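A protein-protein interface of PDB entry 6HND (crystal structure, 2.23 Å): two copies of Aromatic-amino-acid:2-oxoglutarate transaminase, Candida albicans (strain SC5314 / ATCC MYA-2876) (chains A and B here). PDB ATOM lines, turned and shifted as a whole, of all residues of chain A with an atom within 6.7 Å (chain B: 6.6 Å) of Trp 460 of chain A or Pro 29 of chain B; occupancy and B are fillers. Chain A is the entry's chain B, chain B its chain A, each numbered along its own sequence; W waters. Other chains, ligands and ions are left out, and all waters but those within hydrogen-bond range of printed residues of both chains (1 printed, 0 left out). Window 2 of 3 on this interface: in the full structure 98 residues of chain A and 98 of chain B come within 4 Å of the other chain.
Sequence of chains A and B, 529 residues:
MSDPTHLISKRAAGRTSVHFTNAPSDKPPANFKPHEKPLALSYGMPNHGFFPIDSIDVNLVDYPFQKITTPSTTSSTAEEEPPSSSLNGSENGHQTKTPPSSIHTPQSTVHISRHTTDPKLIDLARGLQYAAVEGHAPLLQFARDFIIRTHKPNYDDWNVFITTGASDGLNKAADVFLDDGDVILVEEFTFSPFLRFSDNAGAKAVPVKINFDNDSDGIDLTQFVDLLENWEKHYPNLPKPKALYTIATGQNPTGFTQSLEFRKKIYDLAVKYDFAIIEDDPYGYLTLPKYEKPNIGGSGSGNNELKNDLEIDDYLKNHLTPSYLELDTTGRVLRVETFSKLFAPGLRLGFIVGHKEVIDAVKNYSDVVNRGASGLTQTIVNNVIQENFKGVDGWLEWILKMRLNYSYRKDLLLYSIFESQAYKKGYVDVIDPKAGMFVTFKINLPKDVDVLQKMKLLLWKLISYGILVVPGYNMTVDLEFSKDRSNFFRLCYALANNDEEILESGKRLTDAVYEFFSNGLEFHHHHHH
Trp 460 of chain A touches four residues of chain B.
Of chain A, only Trp 460 (3.5 Å) and Phe 523 (3.7 Å) come within 4 Å of Pro 29 of chain B.
Of the printed residues of chain A, Asn 31 of chain B touches Phe 523.
Of the printed residues of chain A, Lys 33 of chain B touches Ser 464.
The nearest residue of chain A that does not touch Pro 29 of chain B is Leu 457 of chain A (4.5 Å).
The backbone carbonyl oxygen (O) of Lys 461 of chain A sits at hydrogen-bond distance from the side-chain hydroxyl (OG) of Ser 464 of chain A, at 2.6 Å.
O of Trp 460 of chain A sits at hydrogen-bond distance from OG of Ser 464 of chain A.
NZ of Lys 461 of chain A is in hydrogen-bond range of O of Phe 523 of chain A, 2.8 Å away.
Water W1 bridges the backbone carbonyl oxygen (O) of His 524 of chain A (2.7 Å) and the backbone NH (N) of Asn 31 of chain B (3.2 Å).
No position is printed for both chains.
Of the 10 pairs that touch across the chains among the printed residues, none has its exchanged pair printed and touching as well.
Pro 28 of chain B touches Trp 460 of chain A.
Pro 29 of chain B touches Trp 460 of chain A.
Trp 460 of chain A touches Phe 32 of chain B.
Ile 463 of chain A touches Phe 32 of chain B (CG2 to CZ, 3.7 Å).
N of Ser 464 of chain A touches CE1 of Phe 32 of chain B, at 3.9 Å.
Ser 464 of chain A touches Lys 33 of chain B.
Pro 29 of chain B touches Phe 523 of chain A.
Phe 523 of chain A touches Asn 31 of chain B.
Phe 32 of chain B touches Phe 523 of chain A (CD1 to CZ, 3.9 Å).
Hydrophobic or aromatic side chains of chain A that line the printed part of chain B: Trp 460, Ile 463 and Phe 523.
Hydrophobic or aromatic side chains of chain B within 4 Å of the printed part of chain A: Pro 28, Pro 29 and Phe 32.
Among the printed residues, no Asp or Glu carboxylate lies within 4 Å of a Lys or Arg side-chain nitrogen of the other chain.
NE1 of Trp 460 of chain A sits at hydrogen-bond distance from OD1 of Asp 26 of chain B (3.0 Å).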
ATOM      1  N   MET A 455       1.960 -12.637 -18.742  1.00  0.00           N
ATOM      2  CA  MET A 455       0.494 -12.523 -18.536  1.00  0.00           C
ATOM      3  C   MET A 455       0.242 -11.514 -17.406  1.00  0.00           C
ATOM      4  O   MET A 455      -0.677 -10.708 -17.568  1.00  0.00           O
ATOM      5  CB  MET A 455      -0.149 -13.888 -18.242  1.00  0.00           C
ATOM      6  CG  MET A 455      -0.234 -14.803 -19.481  1.00  0.00           C
ATOM      7  SD  MET A 455      -1.280 -14.144 -20.832  1.00  0.00           S
ATOM      8  CE  MET A 455      -2.868 -14.115 -20.003  1.00  0.00           C
ATOM      9  N   LYS A 456       1.065 -11.496 -16.349  1.00  0.00           N
ATOM     10  CA  LYS A 456       0.917 -10.521 -15.219  1.00  0.00           C
ATOM     11  C   LYS A 456       1.197  -9.101 -15.723  1.00  0.00           C
ATOM     12  O   LYS A 456       0.437  -8.198 -15.389  1.00  0.00           O
ATOM     13  CB  LYS A 456       1.823 -10.853 -14.031  1.00  0.00           C
ATOM     14  CG  LYS A 456       1.388 -12.054 -13.216  1.00  0.00           C
ATOM     15  CD  LYS A 456       2.508 -12.651 -12.375  1.00  0.00           C
ATOM     16  CE  LYS A 456       2.094 -13.943 -11.692  1.00  0.00           C
ATOM     17  NZ  LYS A 456       3.253 -14.610 -11.049  1.00  0.00           N
ATOM     18  N   LEU A 457       2.234  -8.938 -16.533  1.00  0.00           N
ATOM     19  CA  LEU A 457       2.622  -7.639 -17.125  1.00  0.00           C
ATOM     20  C   LEU A 457       1.479  -7.148 -18.020  1.00  0.00           C
ATOM     21  O   LEU A 457       1.108  -5.969 -17.901  1.00  0.00           O
ATOM     22  CB  LEU A 457       3.928  -7.840 -17.901  1.00  0.00           C
ATOM     23  CG  LEU A 457       4.803  -6.598 -18.042  1.00  0.00           C
ATOM     24  CD1 LEU A 457       5.106  -5.996 -16.680  1.00  0.00           C
ATOM     25  CD2 LEU A 457       6.081  -6.921 -18.793  1.00  0.00           C
ATOM     26  N   LEU A 458       0.888  -8.052 -18.816  1.00  0.00           N
ATOM     27  CA  LEU A 458      -0.246  -7.741 -19.725  1.00  0.00           C
ATOM     28  C   LEU A 458      -1.472  -7.361 -18.890  1.00  0.00           C
ATOM     29  O   LEU A 458      -2.221  -6.443 -19.303  1.00  0.00           O
ATOM     30  CB  LEU A 458      -0.512  -8.947 -20.632  1.00  0.00           C
ATOM     31  CG  LEU A 458      -1.658  -8.806 -21.628  1.00  0.00           C
ATOM     32  CD1 LEU A 458      -1.567  -7.501 -22.408  1.00  0.00           C
ATOM     33  CD2 LEU A 458      -1.692  -9.999 -22.584  1.00  0.00           C
ATOM     34  N   LEU A 459      -1.666  -8.008 -17.736  1.00  0.00           N
ATOM     35  CA  LEU A 459      -2.827  -7.698 -16.862  1.00  0.00           C
ATOM     36  C   LEU A 459      -2.724  -6.230 -16.413  1.00  0.00           C
ATOM     37  O   LEU A 459      -3.724  -5.494 -16.569  1.00  0.00           O
ATOM     38  CB  LEU A 459      -2.869  -8.651 -15.666  1.00  0.00           C
ATOM     39  CG  LEU A 459      -4.128  -8.538 -14.797  1.00  0.00           C
ATOM     40  CD1 LEU A 459      -5.387  -8.862 -15.597  1.00  0.00           C
ATOM     41  CD2 LEU A 459      -4.030  -9.430 -13.556  1.00  0.00           C
ATOM     42  N   TRP A 460      -1.556  -5.798 -15.917  1.00  0.00           N
ATOM     43  CA  TRP A 460      -1.337  -4.377 -15.541  1.00  0.00           C
ATOM     44  C   TRP A 460      -1.735  -3.468 -16.715  1.00  0.00           C
ATOM     45  O   TRP A 460      -2.428  -2.478 -16.467  1.00  0.00           O
ATOM     46  CB  TRP A 460       0.106  -4.124 -15.114  1.00  0.00           C
ATOM     47  CG  TRP A 460       0.447  -4.692 -13.780  1.00  0.00           C
ATOM     48  CD1 TRP A 460       1.340  -5.692 -13.508  1.00  0.00           C
ATOM     49  CD2 TRP A 460      -0.106  -4.280 -12.522  1.00  0.00           C
ATOM     50  NE1 TRP A 460       1.385  -5.915 -12.160  1.00  0.00           N
ATOM     51  CE2 TRP A 460       0.504  -5.074 -11.532  1.00  0.00           C
ATOM     52  CE3 TRP A 460      -1.053  -3.325 -12.140  1.00  0.00           C
ATOM     53  CZ2 TRP A 460       0.185  -4.939 -10.182  1.00  0.00           C
ATOM     54  CZ3 TRP A 460      -1.375  -3.201 -10.809  1.00  0.00           C
ATOM     55  CH2 TRP A 460      -0.764  -3.998  -9.845  1.00  0.00           C
ATOM     56  N   LYS A 461      -1.351  -3.816 -17.949  1.00  0.00           N
ATOM     57  CA  LYS A 461      -1.677  -3.034 -19.175  1.00  0.00           C
ATOM     58  C   LYS A 461      -3.201  -2.905 -19.384  1.00  0.00           C
ATOM     59  O   LYS A 461      -3.678  -1.795 -19.713  1.00  0.00           O
ATOM     60  CB  LYS A 461      -1.044  -3.690 -20.404  1.00  0.00           C
ATOM     61  CG  LYS A 461      -0.911  -2.765 -21.596  1.00  0.00           C
ATOM     62  CD  LYS A 461      -0.233  -1.454 -21.228  1.00  0.00           C
ATOM     63  CE  LYS A 461       0.452  -0.791 -22.387  1.00  0.00           C
ATOM     64  NZ  LYS A 461       0.926   0.550 -21.994  1.00  0.00           N
ATOM     65  N   LEU A 462      -3.942  -4.005 -19.245  1.00  0.00           N
ATOM     66  CA  LEU A 462      -5.424  -4.009 -19.382  1.00  0.00           C
ATOM     67  C   LEU A 462      -6.003  -3.066 -18.321  1.00  0.00           C
ATOM     68  O   LEU A 462      -6.860  -2.228 -18.678  1.00  0.00           O
ATOM     69  CB  LEU A 462      -5.992  -5.423 -19.193  1.00  0.00           C
ATOM     70  CG  LEU A 462      -5.551  -6.504 -20.181  1.00  0.00           C
ATOM     71  CD1 LEU A 462      -6.346  -7.760 -19.935  1.00  0.00           C
ATOM     72  CD2 LEU A 462      -5.727  -6.076 -21.610  1.00  0.00           C
ATOM     73  N   ILE A 463      -5.555  -3.193 -17.060  1.00  0.00           N
ATOM     74  CA  ILE A 463      -6.048  -2.337 -15.934  1.00  0.00           C
ATOM     75  C   ILE A 463      -5.805  -0.868 -16.307  1.00  0.00           C
ATOM     76  O   ILE A 463      -6.778  -0.095 -16.247  1.00  0.00           O
ATOM     77  CB  ILE A 463      -5.415  -2.718 -14.586  1.00  0.00           C
ATOM     78  CG1 ILE A 463      -5.780  -4.148 -14.168  1.00  0.00           C
ATOM     79  CG2 ILE A 463      -5.794  -1.700 -13.515  1.00  0.00           C
ATOM     80  CD1 ILE A 463      -4.904  -4.707 -13.069  1.00  0.00           C
ATOM     81  N   SER A 464      -4.606  -0.522 -16.790  1.00  0.00           N
ATOM     82  CA  SER A 464      -4.260   0.856 -17.253  1.00  0.00           C
ATOM     83  C   SER A 464      -5.141   1.269 -18.438  1.00  0.00           C
ATOM     84  O   SER A 464      -5.513   2.449 -18.476  1.00  0.00           O
ATOM     85  CB  SER A 464      -2.791   1.043 -17.551  1.00  0.00           C
ATOM     86  OG  SER A 464      -2.377   0.238 -18.622  1.00  0.00           O
ATOM     87  N   TYR A 465      -5.568   0.340 -19.299  1.00  0.00           N
ATOM     88  CA  TYR A 465      -6.488   0.641 -20.437  1.00  0.00           C
ATOM     89  C   TYR A 465      -7.976   0.646 -20.015  1.00  0.00           C
ATOM     90  O   TYR A 465      -8.822   0.977 -20.866  1.00  0.00           O
ATOM     91  CB  TYR A 465      -6.216  -0.313 -21.603  1.00  0.00           C
ATOM     92  CG  TYR A 465      -5.244   0.219 -22.627  1.00  0.00           C
ATOM     93  CD1 TYR A 465      -3.890   0.355 -22.343  1.00  0.00           C
ATOM     94  CD2 TYR A 465      -5.680   0.575 -23.894  1.00  0.00           C
ATOM     95  CE1 TYR A 465      -2.998   0.842 -23.290  1.00  0.00           C
ATOM     96  CE2 TYR A 465      -4.801   1.038 -24.857  1.00  0.00           C
ATOM     97  CZ  TYR A 465      -3.463   1.187 -24.548  1.00  0.00           C
ATOM     98  OH  TYR A 465      -2.630   1.666 -25.507  1.00  0.00           O
ATOM     99  N   PHE A 523       5.134  -3.286 -20.747  1.00  0.00           N
ATOM    100  CA  PHE A 523       4.134  -2.247 -20.385  1.00  0.00           C
ATOM    101  C   PHE A 523       4.524  -0.927 -21.071  1.00  0.00           C
ATOM    102  O   PHE A 523       3.630  -0.272 -21.656  1.00  0.00           O
ATOM    103  CB  PHE A 523       4.023  -2.126 -18.865  1.00  0.00           C
ATOM    104  CG  PHE A 523       2.950  -1.182 -18.407  1.00  0.00           C
ATOM    105  CD1 PHE A 523       3.185   0.183 -18.363  1.00  0.00           C
ATOM    106  CD2 PHE A 523       1.705  -1.656 -18.031  1.00  0.00           C
ATOM    107  CE1 PHE A 523       2.211   1.055 -17.913  1.00  0.00           C
ATOM    108  CE2 PHE A 523       0.725  -0.782 -17.589  1.00  0.00           C
ATOM    109  CZ  PHE A 523       0.978   0.573 -17.542  1.00  0.00           C
ATOM    110  N   HIS A 524       5.822  -0.588 -20.997  1.00  0.00           N
ATOM    111  CA  HIS A 524       6.491   0.592 -21.613  1.00  0.00           C
ATOM    112  C   HIS A 524       5.781   1.878 -21.143  1.00  0.00           C
ATOM    113  O   HIS A 524       5.791   2.286 -19.951  1.00  0.00           O
ATOM    114  CB  HIS A 524       6.627   0.353 -23.134  1.00  0.00           C
ATOM    115  CG  HIS A 524       6.304   1.528 -24.000  1.00  0.00           C
ATOM    116  ND1 HIS A 524       7.116   1.909 -25.066  1.00  0.00           N
ATOM    117  CD2 HIS A 524       5.260   2.398 -23.990  1.00  0.00           C
ATOM    118  CE1 HIS A 524       6.595   2.971 -25.657  1.00  0.00           C
ATOM    119  NE2 HIS A 524       5.455   3.293 -25.012  1.00  0.00           N
ATOM    120  N   ASP B  26       1.891  -9.001  -7.510  1.00  0.00           N
ATOM    121  CA  ASP B  26       3.286  -8.666  -7.911  1.00  0.00           C
ATOM    122  C   ASP B  26       3.407  -7.139  -8.013  1.00  0.00           C
ATOM    123  O   ASP B  26       2.398  -6.467  -7.852  1.00  0.00           O
ATOM    124  CB  ASP B  26       3.710  -9.388  -9.198  1.00  0.00           C
ATOM    125  CG  ASP B  26       3.196  -8.755 -10.487  1.00  0.00           C
ATOM    126  OD1 ASP B  26       1.981  -8.400 -10.535  1.00  0.00           O
ATOM    127  OD2 ASP B  26       4.009  -8.616 -11.433  1.00  0.00           O
ATOM    128  N   LYS B  27       4.615  -6.626  -8.255  1.00  0.00           N
ATOM    129  CA  LYS B  27       4.974  -5.180  -8.145  1.00  0.00           C
ATOM    130  C   LYS B  27       4.514  -4.439  -9.393  1.00  0.00           C
ATOM    131  O   LYS B  27       4.946  -4.778 -10.483  1.00  0.00           O
ATOM    132  CB  LYS B  27       6.496  -5.023  -8.001  1.00  0.00           C
ATOM    133  CG  LYS B  27       7.029  -3.607  -7.812  1.00  0.00           C
ATOM    134  CD  LYS B  27       8.536  -3.541  -8.023  1.00  0.00           C
ATOM    135  CE  LYS B  27       9.220  -2.368  -7.350  1.00  0.00           C
ATOM    136  NZ  LYS B  27       8.444  -1.108  -7.454  1.00  0.00           N
ATOM    137  N   PRO B  28       3.694  -3.377  -9.274  1.00  0.00           N
ATOM    138  CA  PRO B  28       3.249  -2.618 -10.444  1.00  0.00           C
ATOM    139  C   PRO B  28       4.412  -2.080 -11.258  1.00  0.00           C
ATOM    140  O   PRO B  28       5.437  -1.707 -10.700  1.00  0.00           O
ATOM    141  CB  PRO B  28       2.450  -1.447  -9.866  1.00  0.00           C
ATOM    142  CG  PRO B  28       2.036  -1.942  -8.485  1.00  0.00           C
ATOM    143  CD  PRO B  28       3.179  -2.822  -8.011  1.00  0.00           C
ATOM    144  N   PRO B  29       4.314  -2.046 -12.602  1.00  0.00           N
ATOM    145  CA  PRO B  29       5.383  -1.483 -13.430  1.00  0.00           C
ATOM    146  C   PRO B  29       5.462   0.032 -13.205  1.00  0.00           C
ATOM    147  O   PRO B  29       4.512   0.597 -12.668  1.00  0.00           O
ATOM    148  CB  PRO B  29       4.971  -1.832 -14.869  1.00  0.00           C
ATOM    149  CG  PRO B  29       3.459  -1.961 -14.794  1.00  0.00           C
ATOM    150  CD  PRO B  29       3.167  -2.500 -13.402  1.00  0.00           C
ATOM    151  N   ALA B  30       6.576   0.633 -13.630  1.00  0.00           N
ATOM    152  CA  ALA B  30       6.990   2.018 -13.308  1.00  0.00           C
ATOM    153  C   ALA B  30       5.819   3.001 -13.497  1.00  0.00           C
ATOM    154  O   ALA B  30       5.349   3.597 -12.486  1.00  0.00           O
ATOM    155  CB  ALA B  30       8.183   2.393 -14.159  1.00  0.00           C
ATOM    156  N   ASN B  31       5.367   3.189 -14.738  1.00  0.00           N
ATOM    157  CA  ASN B  31       4.535   4.368 -15.098  1.00  0.00           C
ATOM    158  C   ASN B  31       3.072   3.937 -15.197  1.00  0.00           C
ATOM    159  O   ASN B  31       2.410   4.266 -16.215  1.00  0.00           O
ATOM    160  CB  ASN B  31       5.059   5.075 -16.353  1.00  0.00           C
ATOM    161  CG  ASN B  31       5.575   6.466 -16.044  1.00  0.00           C
ATOM    162  OD1 ASN B  31       5.008   7.459 -16.504  1.00  0.00           O
ATOM    163  ND2 ASN B  31       6.620   6.543 -15.233  1.00  0.00           N
ATOM    164  N   PHE B  32       2.593   3.258 -14.150  1.00  0.00           N
ATOM    165  CA  PHE B  32       1.271   2.589 -14.105  1.00  0.00           C
ATOM    166  C   PHE B  32       0.255   3.504 -13.419  1.00  0.00           C
ATOM    167  O   PHE B  32       0.302   3.672 -12.202  1.00  0.00           O
ATOM    168  CB  PHE B  32       1.340   1.239 -13.381  1.00  0.00           C
ATOM    169  CG  PHE B  32      -0.030   0.706 -13.058  1.00  0.00           C
ATOM    170  CD1 PHE B  32      -0.903   0.351 -14.076  1.00  0.00           C
ATOM    171  CD2 PHE B  32      -0.476   0.639 -11.749  1.00  0.00           C
ATOM    172  CE1 PHE B  32      -2.179  -0.103 -13.786  1.00  0.00           C
ATOM    173  CE2 PHE B  32      -1.754   0.192 -11.465  1.00  0.00           C
ATOM    174  CZ  PHE B  32      -2.600  -0.177 -12.481  1.00  0.00           C
ATOM    175  N   LYS B  33      -0.630   4.100 -14.202  1.00  0.00           N
ATOM    176  CA  LYS B  33      -1.834   4.774 -13.675  1.00  0.00           C
ATOM    177  C   LYS B  33      -3.011   3.858 -14.008  1.00  0.00           C
ATOM    178  O   LYS B  33      -3.201   3.471 -15.162  1.00  0.00           O
ATOM    179  CB  LYS B  33      -1.940   6.198 -14.239  1.00  0.00           C
ATOM    180  CG  LYS B  33      -2.783   7.151 -13.395  1.00  0.00           C
ATOM    181  CD  LYS B  33      -2.641   8.637 -13.706  1.00  0.00           C
ATOM    182  CE  LYS B  33      -3.555   9.493 -12.841  1.00  0.00           C
ATOM    183  NZ  LYS B  33      -3.152  10.924 -12.818  1.00  0.00           N
HETATM  184  O   HOH W   1       6.410   1.776 -17.402  1.00  0.00           O
